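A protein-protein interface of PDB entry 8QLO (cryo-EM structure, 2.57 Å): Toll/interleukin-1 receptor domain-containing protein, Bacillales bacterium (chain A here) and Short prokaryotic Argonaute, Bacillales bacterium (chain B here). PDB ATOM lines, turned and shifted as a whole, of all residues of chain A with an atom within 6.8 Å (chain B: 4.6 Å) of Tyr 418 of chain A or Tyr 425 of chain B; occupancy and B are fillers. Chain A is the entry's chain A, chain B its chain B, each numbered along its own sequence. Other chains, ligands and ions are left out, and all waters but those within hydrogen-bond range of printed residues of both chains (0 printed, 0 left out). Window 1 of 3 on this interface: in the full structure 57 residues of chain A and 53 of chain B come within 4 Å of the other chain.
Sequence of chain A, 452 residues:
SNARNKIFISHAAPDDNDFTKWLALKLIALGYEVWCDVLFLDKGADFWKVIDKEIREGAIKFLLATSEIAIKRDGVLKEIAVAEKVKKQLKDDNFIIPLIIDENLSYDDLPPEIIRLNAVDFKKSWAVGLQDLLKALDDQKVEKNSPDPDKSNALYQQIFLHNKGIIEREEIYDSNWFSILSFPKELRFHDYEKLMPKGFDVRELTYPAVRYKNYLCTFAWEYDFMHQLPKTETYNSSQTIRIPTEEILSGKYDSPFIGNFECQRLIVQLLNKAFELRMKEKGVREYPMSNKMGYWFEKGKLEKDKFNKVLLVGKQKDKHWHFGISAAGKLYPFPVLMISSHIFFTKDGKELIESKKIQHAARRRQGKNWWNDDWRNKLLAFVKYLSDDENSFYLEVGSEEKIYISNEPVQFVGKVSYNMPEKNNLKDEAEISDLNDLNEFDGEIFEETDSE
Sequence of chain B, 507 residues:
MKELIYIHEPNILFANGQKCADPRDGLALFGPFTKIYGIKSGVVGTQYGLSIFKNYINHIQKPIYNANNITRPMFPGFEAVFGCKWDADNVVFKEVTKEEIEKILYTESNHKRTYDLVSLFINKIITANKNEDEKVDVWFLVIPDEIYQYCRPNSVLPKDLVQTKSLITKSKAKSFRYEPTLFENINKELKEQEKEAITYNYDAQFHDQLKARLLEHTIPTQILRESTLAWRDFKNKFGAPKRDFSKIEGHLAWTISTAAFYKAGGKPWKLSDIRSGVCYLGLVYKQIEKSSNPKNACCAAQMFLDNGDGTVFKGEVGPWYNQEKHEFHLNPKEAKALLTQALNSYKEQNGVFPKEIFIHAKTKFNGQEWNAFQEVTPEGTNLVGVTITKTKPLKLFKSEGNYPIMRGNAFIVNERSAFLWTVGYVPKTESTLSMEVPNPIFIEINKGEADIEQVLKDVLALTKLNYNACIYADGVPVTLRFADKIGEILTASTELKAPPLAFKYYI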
ATOM      1  N   GLY A 165      -5.667  -9.209 -21.078  1.00  0.00           N
ATOM      2  CA  GLY A 165      -4.420  -9.697 -20.541  1.00  0.00           C
ATOM      3  C   GLY A 165      -3.341  -9.872 -21.598  1.00  0.00           C
ATOM      4  O   GLY A 165      -3.407  -9.347 -22.706  1.00  0.00           O
ATOM      5  N   ILE A 166      -2.320 -10.638 -21.212  1.00  0.00           N
ATOM      6  CA  ILE A 166      -1.198 -10.898 -22.102  1.00  0.00           C
ATOM      7  C   ILE A 166      -1.404 -12.221 -22.829  1.00  0.00           C
ATOM      8  O   ILE A 166      -2.161 -13.094 -22.385  1.00  0.00           O
ATOM      9  CB  ILE A 166       0.125 -10.900 -21.314  1.00  0.00           C
ATOM     10  CG1 ILE A 166       0.209 -12.142 -20.426  1.00  0.00           C
ATOM     11  CG2 ILE A 166       0.244  -9.641 -20.477  1.00  0.00           C
ATOM     12  CD1 ILE A 166       1.615 -12.526 -20.042  1.00  0.00           C
ATOM     13  N   ILE A 167      -0.721 -12.371 -23.961  1.00  0.00           N
ATOM     14  CA  ILE A 167      -0.767 -13.590 -24.757  1.00  0.00           C
ATOM     15  C   ILE A 167       0.657 -14.066 -24.998  1.00  0.00           C
ATOM     16  O   ILE A 167       1.564 -13.267 -25.251  1.00  0.00           O
ATOM     17  CB  ILE A 167      -1.500 -13.388 -26.102  1.00  0.00           C
ATOM     18  CG1 ILE A 167      -2.768 -12.558 -25.906  1.00  0.00           C
ATOM     19  CG2 ILE A 167      -1.835 -14.726 -26.733  1.00  0.00           C
ATOM     20  CD1 ILE A 167      -2.668 -11.165 -26.460  1.00  0.00           C
ATOM     21  N   ARG A 169       2.740 -14.971 -27.290  1.00  0.00           N
ATOM     22  CA  ARG A 169       2.959 -14.911 -28.728  1.00  0.00           C
ATOM     23  C   ARG A 169       4.243 -14.141 -28.985  1.00  0.00           C
ATOM     24  O   ARG A 169       4.395 -13.015 -28.502  1.00  0.00           O
ATOM     25  CB  ARG A 169       1.778 -14.243 -29.438  1.00  0.00           C
ATOM     26  CG  ARG A 169       1.936 -14.119 -30.939  1.00  0.00           C
ATOM     27  CD  ARG A 169       0.804 -13.300 -31.529  1.00  0.00           C
ATOM     28  NE  ARG A 169       0.672 -12.008 -30.866  1.00  0.00           N
ATOM     29  CZ  ARG A 169      -0.428 -11.270 -30.874  1.00  0.00           C
ATOM     30  NH1 ARG A 169      -1.526 -11.673 -31.493  1.00  0.00           N
ATOM     31  NH2 ARG A 169      -0.428 -10.099 -30.245  1.00  0.00           N
ATOM     32  N   GLU A 171       7.026 -11.805 -30.227  1.00  0.00           N
ATOM     33  CA  GLU A 171       6.995 -10.472 -30.814  1.00  0.00           C
ATOM     34  C   GLU A 171       8.420 -10.031 -31.105  1.00  0.00           C
ATOM     35  O   GLU A 171       9.275 -10.061 -30.214  1.00  0.00           O
ATOM     36  CB  GLU A 171       6.305  -9.478 -29.879  1.00  0.00           C
ATOM     37  CG  GLU A 171       6.109  -8.093 -30.473  1.00  0.00           C
ATOM     38  CD  GLU A 171       5.084  -8.072 -31.587  1.00  0.00           C
ATOM     39  OE1 GLU A 171       4.005  -8.675 -31.417  1.00  0.00           O
ATOM     40  OE2 GLU A 171       5.355  -7.446 -32.634  1.00  0.00           O
ATOM     41  N   TYR A 173      10.935  -7.029 -32.101  1.00  0.00           N
ATOM     42  CA  TYR A 173      11.020  -5.589 -31.955  1.00  0.00           C
ATOM     43  C   TYR A 173      12.256  -5.069 -32.671  1.00  0.00           C
ATOM     44  O   TYR A 173      13.327  -5.682 -32.636  1.00  0.00           O
ATOM     45  CB  TYR A 173      11.099  -5.178 -30.479  1.00  0.00           C
ATOM     46  CG  TYR A 173       9.974  -5.684 -29.613  1.00  0.00           C
ATOM     47  CD1 TYR A 173      10.078  -6.901 -28.956  1.00  0.00           C
ATOM     48  CD2 TYR A 173       8.819  -4.940 -29.433  1.00  0.00           C
ATOM     49  CE1 TYR A 173       9.060  -7.368 -28.157  1.00  0.00           C
ATOM     50  CE2 TYR A 173       7.795  -5.400 -28.635  1.00  0.00           C
ATOM     51  CZ  TYR A 173       7.922  -6.614 -27.999  1.00  0.00           C
ATOM     52  OH  TYR A 173       6.904  -7.080 -27.201  1.00  0.00           O
ATOM     53  N   ASN A 372       3.772   4.732 -32.382  1.00  0.00           N
ATOM     54  CA  ASN A 372       4.923   3.793 -32.487  1.00  0.00           C
ATOM     55  C   ASN A 372       5.456   3.755 -33.925  1.00  0.00           C
ATOM     56  O   ASN A 372       6.680   3.919 -34.098  1.00  0.00           O
ATOM     57  CB  ASN A 372       4.543   2.391 -32.008  1.00  0.00           C
ATOM     58  CG  ASN A 372       5.610   1.359 -32.299  1.00  0.00           C
ATOM     59  OD1 ASN A 372       6.720   1.448 -31.781  1.00  0.00           O
ATOM     60  ND2 ASN A 372       5.281   0.368 -33.112  1.00  0.00           N
ATOM     61  N   VAL A 416       6.218 -12.822 -25.144  1.00  0.00           N
ATOM     62  CA  VAL A 416       4.878 -12.386 -24.776  1.00  0.00           C
ATOM     63  C   VAL A 416       4.496 -11.191 -25.634  1.00  0.00           C
ATOM     64  O   VAL A 416       5.348 -10.446 -26.120  1.00  0.00           O
ATOM     65  CB  VAL A 416       4.762 -12.014 -23.282  1.00  0.00           C
ATOM     66  CG1 VAL A 416       4.950 -13.244 -22.408  1.00  0.00           C
ATOM     67  CG2 VAL A 416       5.763 -10.937 -22.932  1.00  0.00           C
ATOM     68  N   SER A 417       3.191 -11.012 -25.811  1.00  0.00           N
ATOM     69  CA  SER A 417       2.672  -9.902 -26.595  1.00  0.00           C
ATOM     70  C   SER A 417       1.233  -9.644 -26.180  1.00  0.00           C
ATOM     71  O   SER A 417       0.596 -10.469 -25.521  1.00  0.00           O
ATOM     72  CB  SER A 417       2.766 -10.182 -28.097  1.00  0.00           C
ATOM     73  OG  SER A 417       2.756  -8.976 -28.838  1.00  0.00           O
ATOM     74  N   TYR A 418       0.728  -8.481 -26.576  1.00  0.00           N
ATOM     75  CA  TYR A 418      -0.649  -8.094 -26.319  1.00  0.00           C
ATOM     76  C   TYR A 418      -1.430  -8.066 -27.624  1.00  0.00           C
ATOM     77  O   TYR A 418      -0.844  -8.068 -28.710  1.00  0.00           O
ATOM     78  CB  TYR A 418      -0.725  -6.725 -25.641  1.00  0.00           C
ATOM     79  CG  TYR A 418      -0.075  -5.609 -26.420  1.00  0.00           C
ATOM     80  CD1 TYR A 418      -0.794  -4.874 -27.350  1.00  0.00           C
ATOM     81  CD2 TYR A 418       1.256  -5.284 -26.221  1.00  0.00           C
ATOM     82  CE1 TYR A 418      -0.206  -3.850 -28.057  1.00  0.00           C
ATOM     83  CE2 TYR A 418       1.852  -4.263 -26.924  1.00  0.00           C
ATOM     84  CZ  TYR A 418       1.117  -3.548 -27.840  1.00  0.00           C
ATOM     85  OH  TYR A 418       1.711  -2.530 -28.543  1.00  0.00           O
ATOM     86  N   ASN A 419      -2.752  -8.042 -27.508  1.00  0.00           N
ATOM     87  CA  ASN A 419      -3.629  -7.971 -28.664  1.00  0.00           C
ATOM     88  C   ASN A 419      -4.048  -6.526 -28.898  1.00  0.00           C
ATOM     89  O   ASN A 419      -4.272  -5.773 -27.948  1.00  0.00           O
ATOM     90  CB  ASN A 419      -4.857  -8.856 -28.459  1.00  0.00           C
ATOM     91  CG  ASN A 419      -4.747 -10.176 -29.190  1.00  0.00           C
ATOM     92  OD1 ASN A 419      -3.841 -10.377 -29.996  1.00  0.00           O
ATOM     93  ND2 ASN A 419      -5.665 -11.090 -28.902  1.00  0.00           N
ATOM     94  N   MET A 420      -4.142  -6.146 -30.167  1.00  0.00           N
ATOM     95  CA  MET A 420      -4.419  -4.762 -30.508  1.00  0.00           C
ATOM     96  C   MET A 420      -5.811  -4.356 -30.023  1.00  0.00           C
ATOM     97  O   MET A 420      -6.758  -5.142 -30.099  1.00  0.00           O
ATOM     98  CB  MET A 420      -4.314  -4.556 -32.015  1.00  0.00           C
ATOM     99  CG  MET A 420      -2.938  -4.867 -32.585  1.00  0.00           C
ATOM    100  SD  MET A 420      -1.705  -3.606 -32.218  1.00  0.00           S
ATOM    101  CE  MET A 420      -2.656  -2.117 -32.504  1.00  0.00           C
ATOM    102  N   PRO A 421      -5.954  -3.138 -29.510  1.00  0.00           N
ATOM    103  CA  PRO A 421      -7.267  -2.682 -29.045  1.00  0.00           C
ATOM    104  C   PRO A 421      -8.269  -2.592 -30.184  1.00  0.00           C
ATOM    105  O   PRO A 421      -7.921  -2.316 -31.334  1.00  0.00           O
ATOM    106  CB  PRO A 421      -6.976  -1.294 -28.462  1.00  0.00           C
ATOM    107  CG  PRO A 421      -5.524  -1.310 -28.153  1.00  0.00           C
ATOM    108  CD  PRO A 421      -4.898  -2.158 -29.216  1.00  0.00           C
ATOM    109  N   LYS B 398       7.967  -1.480 -31.940  1.00  0.00           N
ATOM    110  CA  LYS B 398       7.152  -2.606 -32.364  1.00  0.00           C
ATOM    111  C   LYS B 398       7.067  -2.604 -33.883  1.00  0.00           C
ATOM    112  O   LYS B 398       6.970  -1.542 -34.505  1.00  0.00           O
ATOM    113  CB  LYS B 398       5.755  -2.540 -31.747  1.00  0.00           C
ATOM    114  CG  LYS B 398       5.136  -3.902 -31.499  1.00  0.00           C
ATOM    115  CD  LYS B 398       3.817  -3.786 -30.761  1.00  0.00           C
ATOM    116  CE  LYS B 398       3.370  -5.137 -30.232  1.00  0.00           C
ATOM    117  NZ  LYS B 398       2.469  -5.834 -31.189  1.00  0.00           N
ATOM    118  N   TYR B 403       0.743   1.020 -31.389  1.00  0.00           N
ATOM    119  CA  TYR B 403       0.869   0.819 -29.920  1.00  0.00           C
ATOM    120  C   TYR B 403       2.287   0.352 -29.587  1.00  0.00           C
ATOM    121  O   TYR B 403       2.862  -0.480 -30.324  1.00  0.00           O
ATOM    122  CB  TYR B 403      -0.256  -0.121 -29.476  1.00  0.00           C
ATOM    123  CG  TYR B 403      -1.581   0.603 -29.290  1.00  0.00           C
ATOM    124  CD1 TYR B 403      -1.769   1.493 -28.239  1.00  0.00           C
ATOM    125  CD2 TYR B 403      -2.624   0.437 -30.191  1.00  0.00           C
ATOM    126  CE1 TYR B 403      -2.968   2.163 -28.068  1.00  0.00           C
ATOM    127  CE2 TYR B 403      -3.826   1.108 -30.036  1.00  0.00           C
ATOM    128  CZ  TYR B 403      -3.999   1.974 -28.971  1.00  0.00           C
ATOM    129  OH  TYR B 403      -5.182   2.637 -28.813  1.00  0.00           O
ATOM    130  N   PRO B 404       2.887   0.868 -28.493  1.00  0.00           N
ATOM    131  CA  PRO B 404       4.240   0.517 -28.126  1.00  0.00           C
ATOM    132  C   PRO B 404       4.479  -0.813 -27.445  1.00  0.00           C
ATOM    133  O   PRO B 404       3.592  -1.576 -27.429  1.00  0.00           O
ATOM    134  CB  PRO B 404       4.485   1.559 -27.066  1.00  0.00           C
ATOM    135  CG  PRO B 404       3.172   1.724 -26.416  1.00  0.00           C
ATOM    136  CD  PRO B 404       2.256   1.833 -27.604  1.00  0.00           C
ATOM    137  N   ILE B 405       5.692  -1.032 -26.925  1.00  0.00           N
ATOM    138  CA  ILE B 405       6.052  -2.330 -26.281  1.00  0.00           C
ATOM    139  C   ILE B 405       5.304  -2.453 -24.948  1.00  0.00           C
ATOM    140  O   ILE B 405       5.042  -1.408 -24.318  1.00  0.00           O
ATOM    141  CB  ILE B 405       7.581  -2.432 -26.110  1.00  0.00           C
ATOM    142  CG1 ILE B 405       8.007  -3.736 -25.429  1.00  0.00           C
ATOM    143  CG2 ILE B 405       8.125  -1.214 -25.379  1.00  0.00           C
ATOM    144  CD1 ILE B 405       9.497  -3.855 -25.214  1.00  0.00           C
ATOM    145  N   MET B 406       4.972  -3.683 -24.543  1.00  0.00           N
ATOM    146  CA  MET B 406       4.233  -3.912 -23.273  1.00  0.00           C
ATOM    147  C   MET B 406       5.123  -3.563 -22.077  1.00  0.00           C
ATOM    148  O   MET B 406       6.347  -3.788 -22.166  1.00  0.00           O
ATOM    149  CB  MET B 406       3.808  -5.378 -23.148  1.00  0.00           C
ATOM    150  CG  MET B 406       2.308  -5.574 -23.081  1.00  0.00           C
ATOM    151  SD  MET B 406       1.872  -7.315 -22.847  1.00  0.00           S
ATOM    152  CE  MET B 406       3.373  -8.106 -23.422  1.00  0.00           C
ATOM    153  N   ARG B 407       4.528  -3.043 -20.999  1.00  0.00           N
ATOM    154  CA  ARG B 407       5.299  -2.760 -19.759  1.00  0.00           C
ATOM    155  C   ARG B 407       5.644  -4.094 -19.090  1.00  0.00           C
ATOM    156  O   ARG B 407       4.820  -5.026 -19.182  1.00  0.00           O
ATOM    157  CB  ARG B 407       4.485  -1.870 -18.815  1.00  0.00           C
ATOM    158  CG  ARG B 407       5.214  -1.511 -17.527  1.00  0.00           C
ATOM    159  CD  ARG B 407       4.442  -0.612 -16.584  1.00  0.00           C
ATOM    160  NE  ARG B 407       5.227  -0.334 -15.390  1.00  0.00           N
ATOM    161  CZ  ARG B 407       5.264  -1.109 -14.313  1.00  0.00           C
ATOM    162  NH1 ARG B 407       4.456  -2.149 -14.216  1.00  0.00           N
ATOM    163  NH2 ARG B 407       6.109  -0.837 -13.333  1.00  0.00           N
ATOM    164  N   GLY B 424       5.223   1.951 -20.720  1.00  0.00           N
ATOM    165  CA  GLY B 424       4.923   0.992 -21.789  1.00  0.00           C
ATOM    166  C   GLY B 424       3.463   0.969 -22.179  1.00  0.00           C
ATOM    167  O   GLY B 424       2.845   2.028 -22.187  1.00  0.00           O
ATOM    168  N   TYR B 425       2.969  -0.208 -22.539  1.00  0.00           N
ATOM    169  CA  TYR B 425       1.557  -0.372 -22.925  1.00  0.00           C
ATOM    170  C   TYR B 425       0.991  -1.343 -21.976  1.00  0.00           C
ATOM    171  O   TYR B 425       1.581  -2.408 -21.811  1.00  0.00           O
ATOM    172  CB  TYR B 425       1.352  -1.079 -24.257  1.00  0.00           C
ATOM    173  CG  TYR B 425      -0.083  -1.374 -24.655  1.00  0.00           C
ATOM    174  CD1 TYR B 425      -0.963  -0.359 -24.995  1.00  0.00           C
ATOM    175  CD2 TYR B 425      -0.551  -2.675 -24.663  1.00  0.00           C
ATOM    176  CE1 TYR B 425      -2.271  -0.635 -25.347  1.00  0.00           C
ATOM    177  CE2 TYR B 425      -1.856  -2.965 -25.007  1.00  0.00           C
ATOM    178  CZ  TYR B 425      -2.714  -1.942 -25.351  1.00  0.00           C
ATOM    179  OH  TYR B 425      -3.990  -2.262 -25.683  1.00  0.00           O
ATOM    180  N   VAL B 426      -0.149  -1.009 -21.401  1.00  0.00           N
ATOM    181  CA  VAL B 426      -0.819  -1.866 -20.428  1.00  0.00           C
ATOM    182  C   VAL B 426      -2.019  -2.511 -21.112  1.00  0.00           C
ATOM    183  O   VAL B 426      -2.965  -1.795 -21.473  1.00  0.00           O
ATOM    184  CB  VAL B 426      -1.255  -1.076 -19.189  1.00  0.00           C
ATOM    185  CG1 VAL B 426      -1.440  -2.012 -18.022  1.00  0.00           C
ATOM    186  CG2 VAL B 426      -0.234  -0.007 -18.863  1.00  0.00           C
ATOM    187  N   PRO B 427      -2.024  -3.830 -21.314  1.00  0.00           N
ATOM    188  CA  PRO B 427      -3.200  -4.465 -21.931  1.00  0.00           C
ATOM    189  C   PRO B 427      -4.482  -4.254 -21.149  1.00  0.00           C
ATOM    190  O   PRO B 427      -5.550  -4.104 -21.753  1.00  0.00           O
ATOM    191  CB  PRO B 427      -2.803  -5.947 -21.980  1.00  0.00           C
ATOM    192  CG  PRO B 427      -1.322  -5.935 -21.980  1.00  0.00           C
ATOM    193  CD  PRO B 427      -0.930  -4.788 -21.100  1.00  0.00           C
ATOM    194  N   GLU B 430      -5.481  -0.781 -21.758  1.00  0.00           N
ATOM    195  CA  GLU B 430      -5.424  -0.514 -23.195  1.00  0.00           C
ATOM    196  C   GLU B 430      -4.900   0.894 -23.467  1.00  0.00           C
ATOM    197  O   GLU B 430      -5.410   1.626 -24.316  1.00  0.00           O
ATOM    198  CB  GLU B 430      -6.791  -0.727 -23.843  1.00  0.00           C
ATOM    199  CG  GLU B 430      -7.242  -2.174 -23.857  1.00  0.00           C
ATOM    200  CD  GLU B 430      -8.559  -2.362 -24.577  1.00  0.00           C
ATOM    201  OE1 GLU B 430      -9.174  -1.348 -24.969  1.00  0.00           O
ATOM    202  OE2 GLU B 430      -8.981  -3.524 -24.751  1.00  0.00           O
ATOM    203  N   SER B 431      -3.866   1.272 -22.722  1.00  0.00           N
ATOM    204  CA  SER B 431      -3.303   2.609 -22.820  1.00  0.00           C
ATOM    205  C   SER B 431      -1.818   2.534 -22.507  1.00  0.00           C
ATOM    206  O   SER B 431      -1.267   1.461 -22.250  1.00  0.00           O
ATOM    207  CB  SER B 431      -4.011   3.585 -21.877  1.00  0.00           C
ATOM    208  OG  SER B 431      -3.325   4.822 -21.826  1.00  0.00           O
ATOM    209  N   THR B 432      -1.176   3.697 -22.530  1.00  0.00           N
ATOM    210  CA  THR B 432       0.256   3.812 -22.309  1.00  0.00           C
ATOM    211  C   THR B 432       0.530   4.855 -21.238  1.00  0.00           C
ATOM    212  O   THR B 432      -0.134   5.894 -21.186  1.00  0.00           O
ATOM    213  CB  THR B 432       0.980   4.192 -23.600  1.00  0.00           C
ATOM    214  OG1 THR B 432       0.226   5.198 -24.287  1.00  0.00           O
ATOM    215  CG2 THR B 432       1.109   2.982 -24.498  1.00  0.00           C
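The side-chain amide nitrogen of Asn 372 of chain A sits at hydrogen-bond distance from the backbone carbonyl oxygen of Lys 398 of chain B (2.9 Å).
OE1 of Glu 171 of chain A lies within salt-bridge range of NZ of Lys 398 of chain B, at 3.2 Å.
The side-chain hydroxyl (OH) of Tyr 418 of chain A lies close to the backbone carbonyl oxygen (O) of Pro 404 of chain B.
The backbone carbonyl oxygen of Tyr 403 of chain B sits at hydrogen-bond distance from the side-chain hydroxyl of Tyr 418 of chain A (2.9 Å).
OG of Ser 417 of chain A lies within hydrogen-bond range of OE1 of Glu 171 of chain A (2.9 Å).
The backbone NH (N) of Arg 407 of chain B lies within hydrogen-bond range of the backbone carbonyl oxygen (O) of Tyr 425 of chain B.
NH2 of Arg 169 of chain A lies within hydrogen-bond range of O of Tyr 418 of chain A.
The backbone carbonyl oxygen (O) of Ile 405 of chain B sits at hydrogen-bond distance from the backbone NH (N) of Tyr 425 of chain B, at 3.0 Å.
N of Ile 167 of chain A sits at hydrogen-bond distance from O of Ser 417 of chain A (2.8 Å).
CG2 of Ile 166 of chain A touches SD of Met 406 of chain B, at 3.7 Å.
Ile 405 of chain B touches Tyr 173 of chain A (CG1 to CE2, 3.6 Å).
CB of Asn 372 of chain A touches O of Tyr 403 of chain B (3.7 Å).
Lys 398 of chain B touches Ser 417 of chain A (NZ to OG, 3.9 Å).
Met 406 of chain B touches Tyr 418 of chain A.
CE2 of Tyr 425 of chain B touches CD1 of Tyr 418 of chain A, at 3.2 Å.
Pro 427 of chain B touches Tyr 418 of chain A.
Tyr 403 of chain B touches Met 420 of chain A (CD2 to CE, 3.4 Å).
CG of Pro 421 of chain A touches CE2 of Tyr 403 of chain B, at 3.5 Å.
Pro 421 of chain A touches Tyr 425 of chain B (CG to OH, 3.1 Å).
Tyr 418 of chain A touches just these residues of chain B: Lys 398, Tyr 403, Pro 404, Met 406, Tyr 425 and Pro 427.
Of the printed residues of chain A, Tyr 425 of chain B touches Tyr 418 (3.2 Å) and Pro 421 (3.1 Å).
Of the printed residues of chain A, Tyr 403 of chain B touches Asn 372 (3.7 Å), Tyr 418 (2.9 Å), Met 420 (3.4 Å) and Pro 421 (3.5 Å).
Printed residues of chain B within 4 Å of Asn 372 of chain A: Lys 398 (2.9 Å) and Tyr 403 (3.7 Å).
Printed residues of chain B within 4 Å of Ser 417 of chain A: Lys 398 and Met 406.
Of the printed residues of chain A, Ile 405 of chain B touches Tyr 173 (3.6 Å).
Of the 13 printed residues of chain A, 10 touch a printed residue of chain B.
Printed residues of chain A that touch a printed residue of chain B: Gly 165, Ile 166, Glu 171, Tyr 173, Asn 372, Val 416, Ser 417, Tyr 418, Met 420 and Pro 421.
Printed residues of chain B that touch a printed residue of chain A: Lys 398, Tyr 403, Pro 404, Ile 405, Met 406, Tyr 425 and Pro 427.
Among the printed residues, Asp or Glu carboxylates within 4 Å of a Lys or Arg side-chain nitrogen of the other chain: Glu 171 of chain A with Lys 398 of chain B (3.2 Å).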
